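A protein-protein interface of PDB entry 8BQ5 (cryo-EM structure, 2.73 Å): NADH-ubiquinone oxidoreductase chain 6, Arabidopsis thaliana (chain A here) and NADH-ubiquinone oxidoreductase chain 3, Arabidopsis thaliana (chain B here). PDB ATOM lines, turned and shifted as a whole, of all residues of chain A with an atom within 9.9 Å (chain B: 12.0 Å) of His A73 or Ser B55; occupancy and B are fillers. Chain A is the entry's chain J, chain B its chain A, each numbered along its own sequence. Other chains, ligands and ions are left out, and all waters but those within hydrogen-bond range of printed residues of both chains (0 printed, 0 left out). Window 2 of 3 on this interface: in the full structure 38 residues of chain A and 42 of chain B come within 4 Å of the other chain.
The backbone NH of Ser B55 sits close to a ring nitrogen (ND1) of His A73.
The backbone carbonyl oxygen of Met A71 sits at hydrogen-bond distance from a ring nitrogen (ND1) of His A73.
Among the printed residues, pairs that only touch across the chains: Phe A72 with Phe B57 (3.4 Å), Met A71 with Asp B58 (3.5 Å), Met A71 with Phe B57 (3.6 Å), Phe A67 with Phe B61 (3.8 Å), Met A71 with Phe B61 (3.8 Å), Val A68 with Phe B57 (3.9 Å) and Met A71 with Arg B56 (3.9 Å).
Leu A66 touches none of the printed residues of chain B.
Printed residues of chain B within 4 Å of Val A68: Phe B57 (3.9 Å).
No residue of chain B comes within 4 Å of Gln A75.
Ile A76 touches none of the printed residues of chain B.
Ser B55 touches just one residue of chain A: His A73 (3.0 Å).
Arg B56 touches just one residue of chain A: Met A71.
Of the printed residues of chain A, Phe B57 touches Val A68, Met A71 and Phe A72.
Of the 18 printed residues of chain A, 5 touch a printed residue of chain B.
Hydrophobic or aromatic side chains of chain A that line the printed part of chain B: Phe A67, Met A71, Phe A72 and His A73.
Along chain A the printed residues that touch a printed residue of chain B span positions 67 to 73.
Of the 6 printed residues of chain B, 5 touch a printed residue of chain A.
Printed residues of chain B that touch a printed residue of chain A: Ser B55, Arg B56, Phe B57, Asp B58 and Phe B61.
Hydrophobic or aromatic side chains of chain B within 4 Å of the printed part of chain A: Phe B57 and Phe B61.
Among the printed residues, 8 pairs touch across the chains.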
ATOM      1  N   ASN A  22      25.772 -31.170  30.141  1.00  0.00           N
ATOM      2  CA  ASN A  22      26.565 -29.925  29.941  1.00  0.00           C
ATOM      3  C   ASN A  22      25.980 -29.117  28.769  1.00  0.00           C
ATOM      4  O   ASN A  22      25.922 -29.634  27.655  1.00  0.00           O
ATOM      5  CB  ASN A  22      28.051 -30.242  29.784  1.00  0.00           C
ATOM      6  CG  ASN A  22      28.977 -29.090  30.097  1.00  0.00           C
ATOM      7  OD1 ASN A  22      28.737 -27.953  29.700  1.00  0.00           O
ATOM      8  ND2 ASN A  22      30.058 -29.383  30.797  1.00  0.00           N
ATOM      9  N   PRO A  23      25.501 -27.874  28.996  1.00  0.00           N
ATOM     10  CA  PRO A  23      24.912 -27.059  27.915  1.00  0.00           C
ATOM     11  C   PRO A  23      25.848 -26.806  26.739  1.00  0.00           C
ATOM     12  O   PRO A  23      25.370 -26.625  25.610  1.00  0.00           O
ATOM     13  CB  PRO A  23      24.525 -25.749  28.621  1.00  0.00           C
ATOM     14  CG  PRO A  23      25.033 -25.849  30.020  1.00  0.00           C
ATOM     15  CD  PRO A  23      25.305 -27.277  30.326  1.00  0.00           C
ATOM     16  N   VAL A  24      27.143 -26.676  27.004  1.00  0.00           N
ATOM     17  CA  VAL A  24      28.130 -26.530  25.896  1.00  0.00           C
ATOM     18  C   VAL A  24      27.971 -27.738  24.973  1.00  0.00           C
ATOM     19  O   VAL A  24      27.911 -27.541  23.761  1.00  0.00           O
ATOM     20  CB  VAL A  24      29.574 -26.401  26.423  1.00  0.00           C
ATOM     21  CG1 VAL A  24      30.610 -26.414  25.312  1.00  0.00           C
ATOM     22  CG2 VAL A  24      29.753 -25.185  27.314  1.00  0.00           C
ATOM     23  N   PHE A  65      25.609 -18.747  20.636  1.00  0.00           N
ATOM     24  CA  PHE A  65      25.244 -19.589  21.770  1.00  0.00           C
ATOM     25  C   PHE A  65      26.478 -20.136  22.471  1.00  0.00           C
ATOM     26  O   PHE A  65      26.539 -20.155  23.704  1.00  0.00           O
ATOM     27  CB  PHE A  65      24.346 -20.735  21.315  1.00  0.00           C
ATOM     28  CG  PHE A  65      22.886 -20.425  21.403  1.00  0.00           C
ATOM     29  CD1 PHE A  65      22.176 -20.703  22.558  1.00  0.00           C
ATOM     30  CD2 PHE A  65      22.222 -19.849  20.335  1.00  0.00           C
ATOM     31  CE1 PHE A  65      20.830 -20.414  22.644  1.00  0.00           C
ATOM     32  CE2 PHE A  65      20.878 -19.559  20.414  1.00  0.00           C
ATOM     33  CZ  PHE A  65      20.180 -19.843  21.570  1.00  0.00           C
ATOM     34  N   LEU A  66      27.464 -20.595  21.702  1.00  0.00           N
ATOM     35  CA  LEU A  66      28.667 -21.165  22.294  1.00  0.00           C
ATOM     36  C   LEU A  66      29.439 -20.123  23.088  1.00  0.00           C
ATOM     37  O   LEU A  66      29.866 -20.390  24.216  1.00  0.00           O
ATOM     38  CB  LEU A  66      29.545 -21.771  21.202  1.00  0.00           C
ATOM     39  CG  LEU A  66      30.529 -22.859  21.634  1.00  0.00           C
ATOM     40  CD1 LEU A  66      29.842 -23.949  22.441  1.00  0.00           C
ATOM     41  CD2 LEU A  66      31.237 -23.441  20.426  1.00  0.00           C
ATOM     42  N   PHE A  67      29.616 -18.928  22.520  1.00  0.00           N
ATOM     43  CA  PHE A  67      30.308 -17.858  23.229  1.00  0.00           C
ATOM     44  C   PHE A  67      29.626 -17.554  24.551  1.00  0.00           C
ATOM     45  O   PHE A  67      30.286 -17.436  25.588  1.00  0.00           O
ATOM     46  CB  PHE A  67      30.360 -16.598  22.365  1.00  0.00           C
ATOM     47  CG  PHE A  67      31.602 -16.474  21.541  1.00  0.00           C
ATOM     48  CD1 PHE A  67      32.490 -17.525  21.431  1.00  0.00           C
ATOM     49  CD2 PHE A  67      31.877 -15.300  20.866  1.00  0.00           C
ATOM     50  CE1 PHE A  67      33.631 -17.402  20.667  1.00  0.00           C
ATOM     51  CE2 PHE A  67      33.013 -15.173  20.100  1.00  0.00           C
ATOM     52  CZ  PHE A  67      33.893 -16.224  20.002  1.00  0.00           C
ATOM     53  N   VAL A  68      28.298 -17.424  24.537  1.00  0.00           N
ATOM     54  CA  VAL A  68      27.603 -17.052  25.764  1.00  0.00           C
ATOM     55  C   VAL A  68      27.667 -18.181  26.787  1.00  0.00           C
ATOM     56  O   VAL A  68      28.026 -17.966  27.949  1.00  0.00           O
ATOM     57  CB  VAL A  68      26.152 -16.647  25.461  1.00  0.00           C
ATOM     58  CG1 VAL A  68      25.345 -16.609  26.742  1.00  0.00           C
ATOM     59  CG2 VAL A  68      26.125 -15.298  24.777  1.00  0.00           C
ATOM     60  N   VAL A  69      27.335 -19.404  26.369  1.00  0.00           N
ATOM     61  CA  VAL A  69      27.236 -20.507  27.316  1.00  0.00           C
ATOM     62  C   VAL A  69      28.608 -20.865  27.877  1.00  0.00           C
ATOM     63  O   VAL A  69      28.719 -21.307  29.026  1.00  0.00           O
ATOM     64  CB  VAL A  69      26.541 -21.707  26.644  1.00  0.00           C
ATOM     65  CG1 VAL A  69      26.551 -22.918  27.550  1.00  0.00           C
ATOM     66  CG2 VAL A  69      25.115 -21.342  26.277  1.00  0.00           C
ATOM     67  N   MET A  70      29.678 -20.693  27.108  1.00  0.00           N
ATOM     68  CA  MET A  70      31.039 -20.979  27.633  1.00  0.00           C
ATOM     69  C   MET A  70      31.426 -19.976  28.724  1.00  0.00           C
ATOM     70  O   MET A  70      31.932 -20.421  29.752  1.00  0.00           O
ATOM     71  CB  MET A  70      32.102 -20.979  26.532  1.00  0.00           C
ATOM     72  CG  MET A  70      32.228 -22.315  25.859  1.00  0.00           C
ATOM     73  SD  MET A  70      33.267 -22.184  24.404  1.00  0.00           S
ATOM     74  CE  MET A  70      33.317 -23.894  23.872  1.00  0.00           C
ATOM     75  N   MET A  71      31.171 -18.686  28.513  1.00  0.00           N
ATOM     76  CA  MET A  71      31.562 -17.697  29.508  1.00  0.00           C
ATOM     77  C   MET A  71      30.669 -17.710  30.742  1.00  0.00           C
ATOM     78  O   MET A  71      31.016 -17.077  31.742  1.00  0.00           O
ATOM     79  CB  MET A  71      31.564 -16.303  28.886  1.00  0.00           C
ATOM     80  CG  MET A  71      32.392 -16.196  27.622  1.00  0.00           C
ATOM     81  SD  MET A  71      32.578 -14.488  27.095  1.00  0.00           S
ATOM     82  CE  MET A  71      30.883 -14.087  26.687  1.00  0.00           C
ATOM     83  N   PHE A  72      29.532 -18.405  30.696  1.00  0.00           N
ATOM     84  CA  PHE A  72      28.697 -18.513  31.884  1.00  0.00           C
ATOM     85  C   PHE A  72      29.325 -19.419  32.934  1.00  0.00           C
ATOM     86  O   PHE A  72      29.159 -19.174  34.134  1.00  0.00           O
ATOM     87  CB  PHE A  72      27.307 -19.026  31.510  1.00  0.00           C
ATOM     88  CG  PHE A  72      26.340 -17.940  31.143  1.00  0.00           C
ATOM     89  CD1 PHE A  72      26.628 -16.615  31.414  1.00  0.00           C
ATOM     90  CD2 PHE A  72      25.150 -18.243  30.506  1.00  0.00           C
ATOM     91  CE1 PHE A  72      25.741 -15.616  31.069  1.00  0.00           C
ATOM     92  CE2 PHE A  72      24.263 -17.247  30.158  1.00  0.00           C
ATOM     93  CZ  PHE A  72      24.560 -15.931  30.439  1.00  0.00           C
ATOM     94  N   HIS A  73      30.046 -20.458  32.508  1.00  0.00           N
ATOM     95  CA  HIS A  73      30.629 -21.449  33.413  1.00  0.00           C
ATOM     96  C   HIS A  73      29.567 -22.030  34.344  1.00  0.00           C
ATOM     97  O   HIS A  73      29.686 -21.991  35.569  1.00  0.00           O
ATOM     98  CB  HIS A  73      31.792 -20.853  34.210  1.00  0.00           C
ATOM     99  CG  HIS A  73      32.990 -20.525  33.375  1.00  0.00           C
ATOM    100  ND1 HIS A  73      33.206 -19.272  32.843  1.00  0.00           N
ATOM    101  CD2 HIS A  73      34.036 -21.287  32.981  1.00  0.00           C
ATOM    102  CE1 HIS A  73      34.333 -19.278  32.154  1.00  0.00           C
ATOM    103  NE2 HIS A  73      34.858 -20.488  32.224  1.00  0.00           N
ATOM    104  N   ILE A  74      28.510 -22.572  33.742  1.00  0.00           N
ATOM    105  CA  ILE A  74      27.375 -23.060  34.513  1.00  0.00           C
ATOM    106  C   ILE A  74      27.761 -24.328  35.259  1.00  0.00           C
ATOM    107  O   ILE A  74      28.301 -25.276  34.674  1.00  0.00           O
ATOM    108  CB  ILE A  74      26.168 -23.303  33.598  1.00  0.00           C
ATOM    109  CG1 ILE A  74      25.655 -21.982  33.032  1.00  0.00           C
ATOM    110  CG2 ILE A  74      25.064 -24.003  34.360  1.00  0.00           C
ATOM    111  CD1 ILE A  74      25.317 -22.051  31.570  1.00  0.00           C
ATOM    112  N   GLN A  75      27.482 -24.351  36.559  1.00  0.00           N
ATOM    113  CA  GLN A  75      27.706 -25.535  37.372  1.00  0.00           C
ATOM    114  C   GLN A  75      26.498 -26.458  37.287  1.00  0.00           C
ATOM    115  O   GLN A  75      25.353 -26.000  37.257  1.00  0.00           O
ATOM    116  CB  GLN A  75      27.981 -25.150  38.826  1.00  0.00           C
ATOM    117  CG  GLN A  75      29.465 -25.056  39.210  1.00  0.00           C
ATOM    118  CD  GLN A  75      30.248 -26.359  39.038  1.00  0.00           C
ATOM    119  OE1 GLN A  75      30.175 -27.030  38.007  1.00  0.00           O
ATOM    120  NE2 GLN A  75      31.002 -26.722  40.070  1.00  0.00           N
ATOM    121  N   ILE A  76      26.765 -27.767  37.264  1.00  0.00           N
ATOM    122  CA  ILE A  76      25.721 -28.744  36.967  1.00  0.00           C
ATOM    123  C   ILE A  76      24.613 -28.695  38.009  1.00  0.00           C
ATOM    124  O   ILE A  76      23.465 -29.043  37.719  1.00  0.00           O
ATOM    125  CB  ILE A  76      26.326 -30.158  36.859  1.00  0.00           C
ATOM    126  CG1 ILE A  76      25.695 -30.907  35.694  1.00  0.00           C
ATOM    127  CG2 ILE A  76      26.103 -30.952  38.134  1.00  0.00           C
ATOM    128  CD1 ILE A  76      26.174 -30.406  34.366  1.00  0.00           C
ATOM    129  N   ALA A  77      24.929 -28.248  39.226  1.00  0.00           N
ATOM    130  CA  ALA A  77      23.945 -28.272  40.302  1.00  0.00           C
ATOM    131  C   ALA A  77      22.790 -27.317  40.039  1.00  0.00           C
ATOM    132  O   ALA A  77      21.653 -27.602  40.428  1.00  0.00           O
ATOM    133  CB  ALA A  77      24.619 -27.934  41.632  1.00  0.00           C
ATOM    134  N   GLU A  78      23.053 -26.185  39.387  1.00  0.00           N
ATOM    135  CA  GLU A  78      22.009 -25.190  39.182  1.00  0.00           C
ATOM    136  C   GLU A  78      20.985 -25.601  38.134  1.00  0.00           C
ATOM    137  O   GLU A  78      19.884 -25.041  38.116  1.00  0.00           O
ATOM    138  CB  GLU A  78      22.622 -23.849  38.782  1.00  0.00           C
ATOM    139  CG  GLU A  78      24.044 -23.644  39.255  1.00  0.00           C
ATOM    140  CD  GLU A  78      24.733 -22.514  38.521  1.00  0.00           C
ATOM    141  OE1 GLU A  78      24.224 -21.378  38.579  1.00  0.00           O
ATOM    142  OE2 GLU A  78      25.773 -22.763  37.877  1.00  0.00           O
ATOM    143  N   ILE A  79      21.310 -26.556  37.261  1.00  0.00           N
ATOM    144  CA  ILE A  79      20.425 -26.931  36.167  1.00  0.00           C
ATOM    145  C   ILE A  79      20.075 -28.410  36.166  1.00  0.00           C
ATOM    146  O   ILE A  79      19.297 -28.847  35.318  1.00  0.00           O
ATOM    147  CB  ILE A  79      21.026 -26.532  34.804  1.00  0.00           C
ATOM    148  CG1 ILE A  79      22.457 -27.053  34.687  1.00  0.00           C
ATOM    149  CG2 ILE A  79      20.996 -25.027  34.632  1.00  0.00           C
ATOM    150  CD1 ILE A  79      22.864 -27.379  33.275  1.00  0.00           C
ATOM    151  N   SER B  55      35.206 -18.064  34.793  1.00  0.00           N
ATOM    152  CA  SER B  55      34.245 -17.499  35.731  1.00  0.00           C
ATOM    153  C   SER B  55      34.230 -15.983  35.587  1.00  0.00           C
ATOM    154  O   SER B  55      34.086 -15.249  36.566  1.00  0.00           O
ATOM    155  CB  SER B  55      34.590 -17.912  37.162  1.00  0.00           C
ATOM    156  OG  SER B  55      35.858 -17.408  37.544  1.00  0.00           O
ATOM    157  N   ARG B  56      34.459 -15.537  34.350  1.00  0.00           N
ATOM    158  CA  ARG B  56      34.513 -14.090  34.035  1.00  0.00           C
ATOM    159  C   ARG B  56      33.712 -13.879  32.747  1.00  0.00           C
ATOM    160  O   ARG B  56      34.024 -14.542  31.735  1.00  0.00           O
ATOM    161  CB  ARG B  56      35.977 -13.684  33.856  1.00  0.00           C
ATOM    162  CG  ARG B  56      36.805 -14.705  33.088  1.00  0.00           C
ATOM    163  CD  ARG B  56      38.305 -14.615  33.282  1.00  0.00           C
ATOM    164  NE  ARG B  56      38.684 -14.807  34.674  1.00  0.00           N
ATOM    165  CZ  ARG B  56      38.888 -15.985  35.253  1.00  0.00           C
ATOM    166  NH1 ARG B  56      38.749 -17.104  34.562  1.00  0.00           N
ATOM    167  NH2 ARG B  56      39.232 -16.039  36.526  1.00  0.00           N
ATOM    168  N   PHE B  57      32.680 -13.050  32.793  1.00  0.00           N
ATOM    169  CA  PHE B  57      31.877 -12.744  31.619  1.00  0.00           C
ATOM    170  C   PHE B  57      32.285 -11.393  31.048  1.00  0.00           C
ATOM    171  O   PHE B  57      32.254 -10.378  31.753  1.00  0.00           O
ATOM    172  CB  PHE B  57      30.391 -12.754  31.961  1.00  0.00           C
ATOM    173  CG  PHE B  57      29.513 -12.913  30.763  1.00  0.00           C
ATOM    174  CD1 PHE B  57      29.182 -11.816  29.990  1.00  0.00           C
ATOM    175  CD2 PHE B  57      29.046 -14.158  30.388  1.00  0.00           C
ATOM    176  CE1 PHE B  57      28.386 -11.951  28.878  1.00  0.00           C
ATOM    177  CE2 PHE B  57      28.251 -14.300  29.273  1.00  0.00           C
ATOM    178  CZ  PHE B  57      27.921 -13.195  28.518  1.00  0.00           C
ATOM    179  N   ASP B  58      32.655 -11.380  29.773  1.00  0.00           N
ATOM    180  CA  ASP B  58      32.994 -10.155  29.060  1.00  0.00           C
ATOM    181  C   ASP B  58      31.929  -9.936  27.992  1.00  0.00           C
ATOM    182  O   ASP B  58      31.811 -10.730  27.053  1.00  0.00           O
ATOM    183  CB  ASP B  58      34.395 -10.247  28.460  1.00  0.00           C
ATOM    184  CG  ASP B  58      34.860  -8.939  27.852  1.00  0.00           C
ATOM    185  OD1 ASP B  58      34.139  -7.928  27.971  1.00  0.00           O
ATOM    186  OD2 ASP B  58      35.961  -8.920  27.267  1.00  0.00           O
ATOM    187  N   ILE B  59      31.158  -8.855  28.141  1.00  0.00           N
ATOM    188  CA  ILE B  59      30.025  -8.590  27.262  1.00  0.00           C
ATOM    189  C   ILE B  59      30.453  -8.330  25.829  1.00  0.00           C
ATOM    190  O   ILE B  59      29.633  -8.434  24.912  1.00  0.00           O
ATOM    191  CB  ILE B  59      29.208  -7.391  27.784  1.00  0.00           C
ATOM    192  CG1 ILE B  59      30.088  -6.140  27.836  1.00  0.00           C
ATOM    193  CG2 ILE B  59      28.630  -7.697  29.145  1.00  0.00           C
ATOM    194  CD1 ILE B  59      29.394  -4.877  27.383  1.00  0.00           C
ATOM    195  N   PHE B  61      32.373  -9.982  23.839  1.00  0.00           N
ATOM    196  CA  PHE B  61      32.335 -11.155  22.972  1.00  0.00           C
ATOM    197  C   PHE B  61      30.915 -11.435  22.492  1.00  0.00           C
ATOM    198  O   PHE B  61      30.698 -11.751  21.315  1.00  0.00           O
ATOM    199  CB  PHE B  61      32.924 -12.363  23.701  1.00  0.00           C
ATOM    200  CG  PHE B  61      34.400 -12.248  23.956  1.00  0.00           C
ATOM    201  CD1 PHE B  61      35.302 -12.271  22.904  1.00  0.00           C
ATOM    202  CD2 PHE B  61      34.888 -12.101  25.242  1.00  0.00           C
ATOM    203  CE1 PHE B  61      36.660 -12.155  23.130  1.00  0.00           C
ATOM    204  CE2 PHE B  61      36.246 -11.987  25.475  1.00  0.00           C
ATOM    205  CZ  PHE B  61      37.133 -12.014  24.415  1.00  0.00           C
